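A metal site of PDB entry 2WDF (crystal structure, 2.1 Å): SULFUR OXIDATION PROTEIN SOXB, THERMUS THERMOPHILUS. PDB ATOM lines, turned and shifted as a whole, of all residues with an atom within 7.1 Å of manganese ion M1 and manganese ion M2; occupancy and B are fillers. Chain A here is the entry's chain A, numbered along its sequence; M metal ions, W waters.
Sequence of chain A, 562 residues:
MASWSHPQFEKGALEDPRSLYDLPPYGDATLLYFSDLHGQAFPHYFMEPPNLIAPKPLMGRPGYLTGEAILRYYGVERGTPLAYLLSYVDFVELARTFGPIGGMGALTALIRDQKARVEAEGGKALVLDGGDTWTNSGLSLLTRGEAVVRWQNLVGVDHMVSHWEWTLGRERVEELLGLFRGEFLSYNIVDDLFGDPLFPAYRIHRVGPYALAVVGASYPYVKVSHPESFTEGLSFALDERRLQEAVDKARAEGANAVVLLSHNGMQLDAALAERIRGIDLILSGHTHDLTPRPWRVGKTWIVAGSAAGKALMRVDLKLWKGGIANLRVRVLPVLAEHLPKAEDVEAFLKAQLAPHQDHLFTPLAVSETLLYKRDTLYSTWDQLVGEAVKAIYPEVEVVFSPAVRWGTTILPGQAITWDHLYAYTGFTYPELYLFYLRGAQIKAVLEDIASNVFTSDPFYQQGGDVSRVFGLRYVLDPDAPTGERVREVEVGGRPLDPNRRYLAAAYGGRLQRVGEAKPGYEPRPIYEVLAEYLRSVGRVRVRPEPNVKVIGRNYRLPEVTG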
ATOM      1  N   SER A  35      10.233 -23.718 -29.006  1.00  0.00           N
ATOM      2  CA  SER A  35       9.521 -24.104 -27.820  1.00  0.00           C
ATOM      3  C   SER A  35       8.280 -24.926 -28.161  1.00  0.00           C
ATOM      4  O   SER A  35       7.780 -24.866 -29.276  1.00  0.00           O
ATOM      5  CB  SER A  35       9.095 -22.855 -27.046  1.00  0.00           C
ATOM      6  OG  SER A  35       8.606 -23.191 -25.757  1.00  0.00           O
ATOM      7  N   ASP A  36       7.804 -25.681 -27.183  1.00  0.00           N
ATOM      8  CA  ASP A  36       6.563 -26.416 -27.332  1.00  0.00           C
ATOM      9  C   ASP A  36       6.515 -27.344 -28.548  1.00  0.00           C
ATOM     10  O   ASP A  36       5.504 -27.406 -29.263  1.00  0.00           O
ATOM     11  CB  ASP A  36       5.406 -25.402 -27.391  1.00  0.00           C
ATOM     12  CG  ASP A  36       5.267 -24.611 -26.098  1.00  0.00           C
ATOM     13  OD1 ASP A  36       4.567 -25.107 -25.187  1.00  0.00           O
ATOM     14  OD2 ASP A  36       5.838 -23.506 -25.970  1.00  0.00           O
ATOM     15  N   LEU A  37       7.600 -28.090 -28.740  1.00  0.00           N
ATOM     16  CA  LEU A  37       7.706 -29.070 -29.814  1.00  0.00           C
ATOM     17  C   LEU A  37       6.672 -30.189 -29.584  1.00  0.00           C
ATOM     18  O   LEU A  37       6.114 -30.740 -30.534  1.00  0.00           O
ATOM     19  CB  LEU A  37       9.120 -29.666 -29.845  1.00  0.00           C
ATOM     20  CG  LEU A  37       9.437 -30.707 -30.933  1.00  0.00           C
ATOM     21  CD1 LEU A  37       9.460 -30.087 -32.319  1.00  0.00           C
ATOM     22  CD2 LEU A  37      10.777 -31.382 -30.661  1.00  0.00           C
ATOM     23  N   HIS A  38       6.403 -30.484 -28.321  1.00  0.00           N
ATOM     24  CA  HIS A  38       5.424 -31.536 -27.981  1.00  0.00           C
ATOM     25  C   HIS A  38       5.715 -32.833 -28.730  1.00  0.00           C
ATOM     26  O   HIS A  38       4.847 -33.419 -29.351  1.00  0.00           O
ATOM     27  CB  HIS A  38       3.979 -31.072 -28.191  1.00  0.00           C
ATOM     28  CG  HIS A  38       3.492 -30.148 -27.112  1.00  0.00           C
ATOM     29  ND1 HIS A  38       2.939 -30.617 -25.933  1.00  0.00           N
ATOM     30  CD2 HIS A  38       3.538 -28.809 -26.995  1.00  0.00           C
ATOM     31  CE1 HIS A  38       2.638 -29.587 -25.156  1.00  0.00           C
ATOM     32  NE2 HIS A  38       3.002 -28.473 -25.778  1.00  0.00           N
ATOM     33  N   GLY A 130      12.274 -23.810 -25.070  1.00  0.00           N
ATOM     34  CA  GLY A 130      11.269 -23.285 -24.163  1.00  0.00           C
ATOM     35  C   GLY A 130      10.418 -24.253 -23.356  1.00  0.00           C
ATOM     36  O   GLY A 130       9.617 -23.816 -22.507  1.00  0.00           O
ATOM     37  N   GLY A 131      10.577 -25.560 -23.574  1.00  0.00           N
ATOM     38  CA  GLY A 131       9.832 -26.555 -22.823  1.00  0.00           C
ATOM     39  C   GLY A 131       8.679 -27.202 -23.580  1.00  0.00           C
ATOM     40  O   GLY A 131       8.438 -26.866 -24.749  1.00  0.00           O
ATOM     41  N   ASP A 132       7.973 -28.122 -22.938  1.00  0.00           N
ATOM     42  CA  ASP A 132       6.906 -28.864 -23.594  1.00  0.00           C
ATOM     43  C   ASP A 132       7.470 -29.586 -24.812  1.00  0.00           C
ATOM     44  O   ASP A 132       6.874 -29.615 -25.880  1.00  0.00           O
ATOM     45  CB  ASP A 132       5.743 -27.960 -23.985  1.00  0.00           C
ATOM     46  CG  ASP A 132       4.759 -27.785 -22.858  1.00  0.00           C
ATOM     47  OD1 ASP A 132       5.060 -28.302 -21.760  1.00  0.00           O
ATOM     48  OD2 ASP A 132       3.751 -27.058 -23.028  1.00  0.00           O
ATOM     49  N   THR A 133       8.647 -30.169 -24.600  1.00  0.00           N
ATOM     50  CA  THR A 133       9.382 -30.897 -25.625  1.00  0.00           C
ATOM     51  C   THR A 133       9.205 -32.423 -25.592  1.00  0.00           C
ATOM     52  O   THR A 133       9.021 -33.071 -26.616  1.00  0.00           O
ATOM     53  CB  THR A 133      10.891 -30.590 -25.459  1.00  0.00           C
ATOM     54  OG1 THR A 133      11.062 -29.184 -25.249  1.00  0.00           O
ATOM     55  CG2 THR A 133      11.684 -31.033 -26.664  1.00  0.00           C
ATOM     56  N   ASN A 136       3.718 -35.884 -25.521  1.00  0.00           N
ATOM     57  CA  ASN A 136       2.623 -35.708 -26.483  1.00  0.00           C
ATOM     58  C   ASN A 136       2.848 -36.075 -27.953  1.00  0.00           C
ATOM     59  O   ASN A 136       2.437 -35.345 -28.852  1.00  0.00           O
ATOM     60  CB  ASN A 136       2.028 -34.307 -26.338  1.00  0.00           C
ATOM     61  CG  ASN A 136       1.942 -33.860 -24.884  1.00  0.00           C
ATOM     62  OD1 ASN A 136       2.592 -32.901 -24.475  1.00  0.00           O
ATOM     63  ND2 ASN A 136       1.189 -34.607 -24.075  1.00  0.00           N
ATOM     64  N   SER A 162      10.518 -26.189 -18.473  1.00  0.00           N
ATOM     65  CA  SER A 162       9.533 -27.262 -18.549  1.00  0.00           C
ATOM     66  C   SER A 162       8.090 -26.907 -18.241  1.00  0.00           C
ATOM     67  O   SER A 162       7.784 -25.871 -17.638  1.00  0.00           O
ATOM     68  CB  SER A 162       9.937 -28.366 -17.565  1.00  0.00           C
ATOM     69  OG  SER A 162       9.729 -27.913 -16.226  1.00  0.00           O
ATOM     70  N   HIS A 163       7.217 -27.844 -18.605  1.00  0.00           N
ATOM     71  CA  HIS A 163       5.805 -27.816 -18.273  1.00  0.00           C
ATOM     72  C   HIS A 163       5.284 -29.259 -18.308  1.00  0.00           C
ATOM     73  O   HIS A 163       5.307 -29.956 -17.290  1.00  0.00           O
ATOM     74  CB  HIS A 163       4.984 -26.866 -19.150  1.00  0.00           C
ATOM     75  CG  HIS A 163       3.491 -27.018 -18.962  1.00  0.00           C
ATOM     76  ND1 HIS A 163       2.576 -26.500 -19.848  1.00  0.00           N
ATOM     77  CD2 HIS A 163       2.768 -27.679 -18.028  1.00  0.00           C
ATOM     78  CE1 HIS A 163       1.351 -26.828 -19.469  1.00  0.00           C
ATOM     79  NE2 HIS A 163       1.437 -27.536 -18.362  1.00  0.00           N
ATOM     80  N   TRP A 164       4.877 -29.726 -19.496  1.00  0.00           N
ATOM     81  CA  TRP A 164       4.335 -31.087 -19.679  1.00  0.00           C
ATOM     82  C   TRP A 164       5.317 -32.205 -19.354  1.00  0.00           C
ATOM     83  O   TRP A 164       4.909 -33.356 -19.136  1.00  0.00           O
ATOM     84  CB  TRP A 164       3.749 -31.302 -21.089  1.00  0.00           C
ATOM     85  CG  TRP A 164       2.377 -30.710 -21.247  1.00  0.00           C
ATOM     86  CD1 TRP A 164       2.076 -29.403 -21.480  1.00  0.00           C
ATOM     87  CD2 TRP A 164       1.117 -31.384 -21.109  1.00  0.00           C
ATOM     88  NE1 TRP A 164       0.713 -29.235 -21.530  1.00  0.00           N
ATOM     89  CE2 TRP A 164       0.108 -30.429 -21.276  1.00  0.00           C
ATOM     90  CE3 TRP A 164       0.760 -32.709 -20.815  1.00  0.00           C
ATOM     91  CZ2 TRP A 164      -1.244 -30.745 -21.167  1.00  0.00           C
ATOM     92  CZ3 TRP A 164      -0.573 -33.029 -20.737  1.00  0.00           C
ATOM     93  CH2 TRP A 164      -1.560 -32.063 -20.921  1.00  0.00           C
ATOM     94  N   TYR A 219       6.454 -23.536 -16.014  1.00  0.00           N
ATOM     95  CA  TYR A 219       5.012 -23.234 -15.875  1.00  0.00           C
ATOM     96  C   TYR A 219       4.611 -23.317 -14.405  1.00  0.00           C
ATOM     97  O   TYR A 219       4.809 -24.341 -13.749  1.00  0.00           O
ATOM     98  CB  TYR A 219       4.181 -24.219 -16.713  1.00  0.00           C
ATOM     99  CG  TYR A 219       2.707 -23.866 -16.805  1.00  0.00           C
ATOM    100  CD1 TYR A 219       2.291 -22.649 -17.321  1.00  0.00           C
ATOM    101  CD2 TYR A 219       1.739 -24.752 -16.366  1.00  0.00           C
ATOM    102  CE1 TYR A 219       0.945 -22.319 -17.389  1.00  0.00           C
ATOM    103  CE2 TYR A 219       0.384 -24.434 -16.434  1.00  0.00           C
ATOM    104  CZ  TYR A 219       0.003 -23.216 -16.958  1.00  0.00           C
ATOM    105  OH  TYR A 219      -1.343 -22.937 -17.107  1.00  0.00           O
ATOM    106  N   HIS A 226      -2.435 -30.799 -13.935  1.00  0.00           N
ATOM    107  CA  HIS A 226      -2.176 -32.216 -14.131  1.00  0.00           C
ATOM    108  C   HIS A 226      -2.353 -32.971 -12.816  1.00  0.00           C
ATOM    109  O   HIS A 226      -2.488 -32.358 -11.765  1.00  0.00           O
ATOM    110  CB  HIS A 226      -0.771 -32.406 -14.691  1.00  0.00           C
ATOM    111  CG  HIS A 226      -0.415 -31.403 -15.750  1.00  0.00           C
ATOM    112  ND1 HIS A 226      -0.777 -31.559 -17.068  1.00  0.00           N
ATOM    113  CD2 HIS A 226       0.230 -30.217 -15.670  1.00  0.00           C
ATOM    114  CE1 HIS A 226      -0.357 -30.514 -17.765  1.00  0.00           C
ATOM    115  NE2 HIS A 226       0.254 -29.688 -16.938  1.00  0.00           N
ATOM    116  N   HIS A 263       8.294 -20.329 -19.528  1.00  0.00           N
ATOM    117  CA  HIS A 263       7.164 -21.207 -19.818  1.00  0.00           C
ATOM    118  C   HIS A 263       5.969 -20.815 -18.973  1.00  0.00           C
ATOM    119  O   HIS A 263       5.145 -21.668 -18.591  1.00  0.00           O
ATOM    120  CB  HIS A 263       7.473 -22.707 -19.659  1.00  0.00           C
ATOM    121  CG  HIS A 263       6.590 -23.566 -20.503  1.00  0.00           C
ATOM    122  ND1 HIS A 263       7.015 -24.132 -21.694  1.00  0.00           N
ATOM    123  CD2 HIS A 263       5.260 -23.806 -20.439  1.00  0.00           C
ATOM    124  CE1 HIS A 263       6.001 -24.758 -22.264  1.00  0.00           C
ATOM    125  NE2 HIS A 263       4.925 -24.574 -21.520  1.00  0.00           N
ATOM    126  N   GLY A 285       7.303 -19.186 -24.094  1.00  0.00           N
ATOM    127  CA  GLY A 285       6.721 -20.466 -24.480  1.00  0.00           C
ATOM    128  C   GLY A 285       5.305 -20.577 -23.930  1.00  0.00           C
ATOM    129  O   GLY A 285       4.697 -19.573 -23.551  1.00  0.00           O
ATOM    130  N   HIS A 286       4.761 -21.802 -23.945  1.00  0.00           N
ATOM    131  CA  HIS A 286       3.440 -22.136 -23.398  1.00  0.00           C
ATOM    132  C   HIS A 286       2.179 -21.774 -24.177  1.00  0.00           C
ATOM    133  O   HIS A 286       1.253 -22.585 -24.273  1.00  0.00           O
ATOM    134  CB  HIS A 286       3.275 -21.633 -21.973  1.00  0.00           C
ATOM    135  CG  HIS A 286       2.026 -22.123 -21.314  1.00  0.00           C
ATOM    136  ND1 HIS A 286       1.790 -23.468 -21.088  1.00  0.00           N
ATOM    137  CD2 HIS A 286       0.917 -21.462 -20.898  1.00  0.00           C
ATOM    138  CE1 HIS A 286       0.594 -23.604 -20.520  1.00  0.00           C
ATOM    139  NE2 HIS A 286       0.045 -22.411 -20.396  1.00  0.00           N
ATOM    140  N   THR A 287       2.093 -20.535 -24.646  1.00  0.00           N
ATOM    141  CA  THR A 287       0.919 -20.065 -25.354  1.00  0.00           C
ATOM    142  C   THR A 287       0.900 -20.370 -26.849  1.00  0.00           C
ATOM    143  O   THR A 287      -0.115 -20.151 -27.514  1.00  0.00           O
ATOM    144  CB  THR A 287       0.584 -18.605 -25.020  1.00  0.00           C
ATOM    145  OG1 THR A 287       1.801 -17.843 -24.866  1.00  0.00           O
ATOM    146  CG2 THR A 287      -0.193 -18.547 -23.692  1.00  0.00           C
ATOM    147  N   HIS A 288       2.002 -20.946 -27.343  1.00  0.00           N
ATOM    148  CA  HIS A 288       2.147 -21.353 -28.749  1.00  0.00           C
ATOM    149  C   HIS A 288       2.023 -20.193 -29.743  1.00  0.00           C
ATOM    150  O   HIS A 288       1.599 -20.366 -30.891  1.00  0.00           O
ATOM    151  CB  HIS A 288       1.148 -22.471 -29.091  1.00  0.00           C
ATOM    152  CG  HIS A 288       1.384 -23.734 -28.314  1.00  0.00           C
ATOM    153  ND1 HIS A 288       0.895 -24.959 -28.722  1.00  0.00           N
ATOM    154  CD2 HIS A 288       2.034 -23.964 -27.151  1.00  0.00           C
ATOM    155  CE1 HIS A 288       1.232 -25.883 -27.847  1.00  0.00           C
ATOM    156  NE2 HIS A 288       1.917 -25.308 -26.879  1.00  0.00           N
ATOM    157  N   SER A 306       6.434 -20.246 -30.742  1.00  0.00           N
ATOM    158  CA  SER A 306       5.638 -21.061 -31.656  1.00  0.00           C
ATOM    159  C   SER A 306       5.415 -22.459 -31.070  1.00  0.00           C
ATOM    160  O   SER A 306       5.301 -22.604 -29.845  1.00  0.00           O
ATOM    161  CB  SER A 306       6.265 -21.130 -33.058  1.00  0.00           C
ATOM    162  OG  SER A 306       5.342 -21.610 -34.042  1.00  0.00           O
ATOM    163  N   ALA A 307       5.323 -23.485 -31.922  1.00  0.00           N
ATOM    164  CA  ALA A 307       5.037 -24.826 -31.430  1.00  0.00           C
ATOM    165  C   ALA A 307       5.148 -25.931 -32.472  1.00  0.00           C
ATOM    166  O   ALA A 307       5.107 -25.681 -33.669  1.00  0.00           O
ATOM    167  CB  ALA A 307       3.615 -24.852 -30.853  1.00  0.00           C
ATOM    168  N   ARG A 405      -3.459 -26.609 -26.531  1.00  0.00           N
ATOM    169  CA  ARG A 405      -2.954 -25.928 -27.723  1.00  0.00           C
ATOM    170  C   ARG A 405      -2.006 -26.776 -28.559  1.00  0.00           C
ATOM    171  O   ARG A 405      -1.536 -26.349 -29.609  1.00  0.00           O
ATOM    172  CB  ARG A 405      -2.274 -24.618 -27.334  1.00  0.00           C
ATOM    173  CG  ARG A 405      -3.160 -23.386 -27.552  1.00  0.00           C
ATOM    174  CD  ARG A 405      -3.351 -22.616 -26.253  1.00  0.00           C
ATOM    175  NE  ARG A 405      -2.612 -21.364 -26.270  1.00  0.00           N
ATOM    176  CZ  ARG A 405      -3.172 -20.162 -26.307  1.00  0.00           C
ATOM    177  NH1 ARG A 405      -4.484 -20.045 -26.343  1.00  0.00           N
ATOM    178  NH2 ARG A 405      -2.412 -19.072 -26.315  1.00  0.00           N
ATOM    179  N   TRP A 406      -1.715 -27.991 -28.076  1.00  0.00           N
ATOM    180  CA  TRP A 406      -0.862 -28.887 -28.836  1.00  0.00           C
ATOM    181  C   TRP A 406      -1.739 -29.787 -29.696  1.00  0.00           C
ATOM    182  O   TRP A 406      -2.912 -29.968 -29.402  1.00  0.00           O
ATOM    183  CB  TRP A 406       0.063 -29.732 -27.935  1.00  0.00           C
ATOM    184  CG  TRP A 406      -0.558 -30.340 -26.704  1.00  0.00           C
ATOM    185  CD1 TRP A 406      -0.588 -29.807 -25.453  1.00  0.00           C
ATOM    186  CD2 TRP A 406      -1.031 -31.698 -26.558  1.00  0.00           C
ATOM    187  NE1 TRP A 406      -1.073 -30.723 -24.552  1.00  0.00           N
ATOM    188  CE2 TRP A 406      -1.371 -31.885 -25.215  1.00  0.00           C
ATOM    189  CE3 TRP A 406      -1.272 -32.735 -27.467  1.00  0.00           C
ATOM    190  CZ2 TRP A 406      -1.916 -33.080 -24.731  1.00  0.00           C
ATOM    191  CZ3 TRP A 406      -1.797 -33.936 -26.997  1.00  0.00           C
ATOM    192  CH2 TRP A 406      -2.116 -34.087 -25.639  1.00  0.00           C
HETATM  193 MN    MN M   1       2.842 -26.319 -25.002  1.00  0.00          MN
HETATM  194 MN    MN M   2       2.916 -25.446 -21.768  1.00  0.00          MN
HETATM  195  O   HOH W   1       1.742 -25.337 -23.623  1.00  0.00           O
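Manganese ion M1 is bound by water W1 (2.0 Å), OD1 of Asp 36 (2.1 Å), OD2 of Asp 132 (2.3 Å), NE2 of His 38 (2.3 Å) and NE2 of His 288 (2.3 Å). Manganese ion M1 has five donor atoms within binding distance.
Five residues have an atom within 4 Å of manganese ion M2: Asp 36, Asp 132, His 163, His 263 and His 286. The nearest printed residue that does not touch manganese ion M2 is Trp 164 (4.1 Å).
Manganese ion M2 is bound by water W1, a ring nitrogen (NE2) of His 263, the side-chain carboxylate (OD2) of Asp 132, a ring nitrogen (ND1) of His 163 and a ring nitrogen (ND1) of His 286. Manganese ion M2 has five donor atoms within binding distance.
N of His 286 is in hydrogen-bond range of OD2 of Asp 36 (2.9 Å). The backbone NH of Asp 36 sits at hydrogen-bond distance from the backbone carbonyl oxygen of Gly 131, 2.8 Å away. The side-chain hydroxyl of Ser 35 sits at hydrogen-bond distance from the side-chain carboxylate of Asp 36 (2.8 Å). The side-chain carboxylate of Asp 132 lies within hydrogen-bond range of the backbone NH of Trp 164, 2.7 Å away. O of Asp 132 is in hydrogen-bond range of N of Leu 37. NE2 of His 226 lies within hydrogen-bond range of NE2 of His 163 (2.8 Å). A ring nitrogen (ND1) of His 38 sits at hydrogen-bond distance from the side-chain amide oxygen of Asn 136 (2.7 Å). The backbone carbonyl oxygen of Arg 405 lies within hydrogen-bond range of a ring nitrogen (ND1) of His 288 (2.9 Å).
Four residues have an atom within 4 Å of manganese ion M1: Asp 36, His 38, Asp 132 and His 288. Along chain A the residues within 4 Å of manganese ion M1 span positions 36 to 288.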
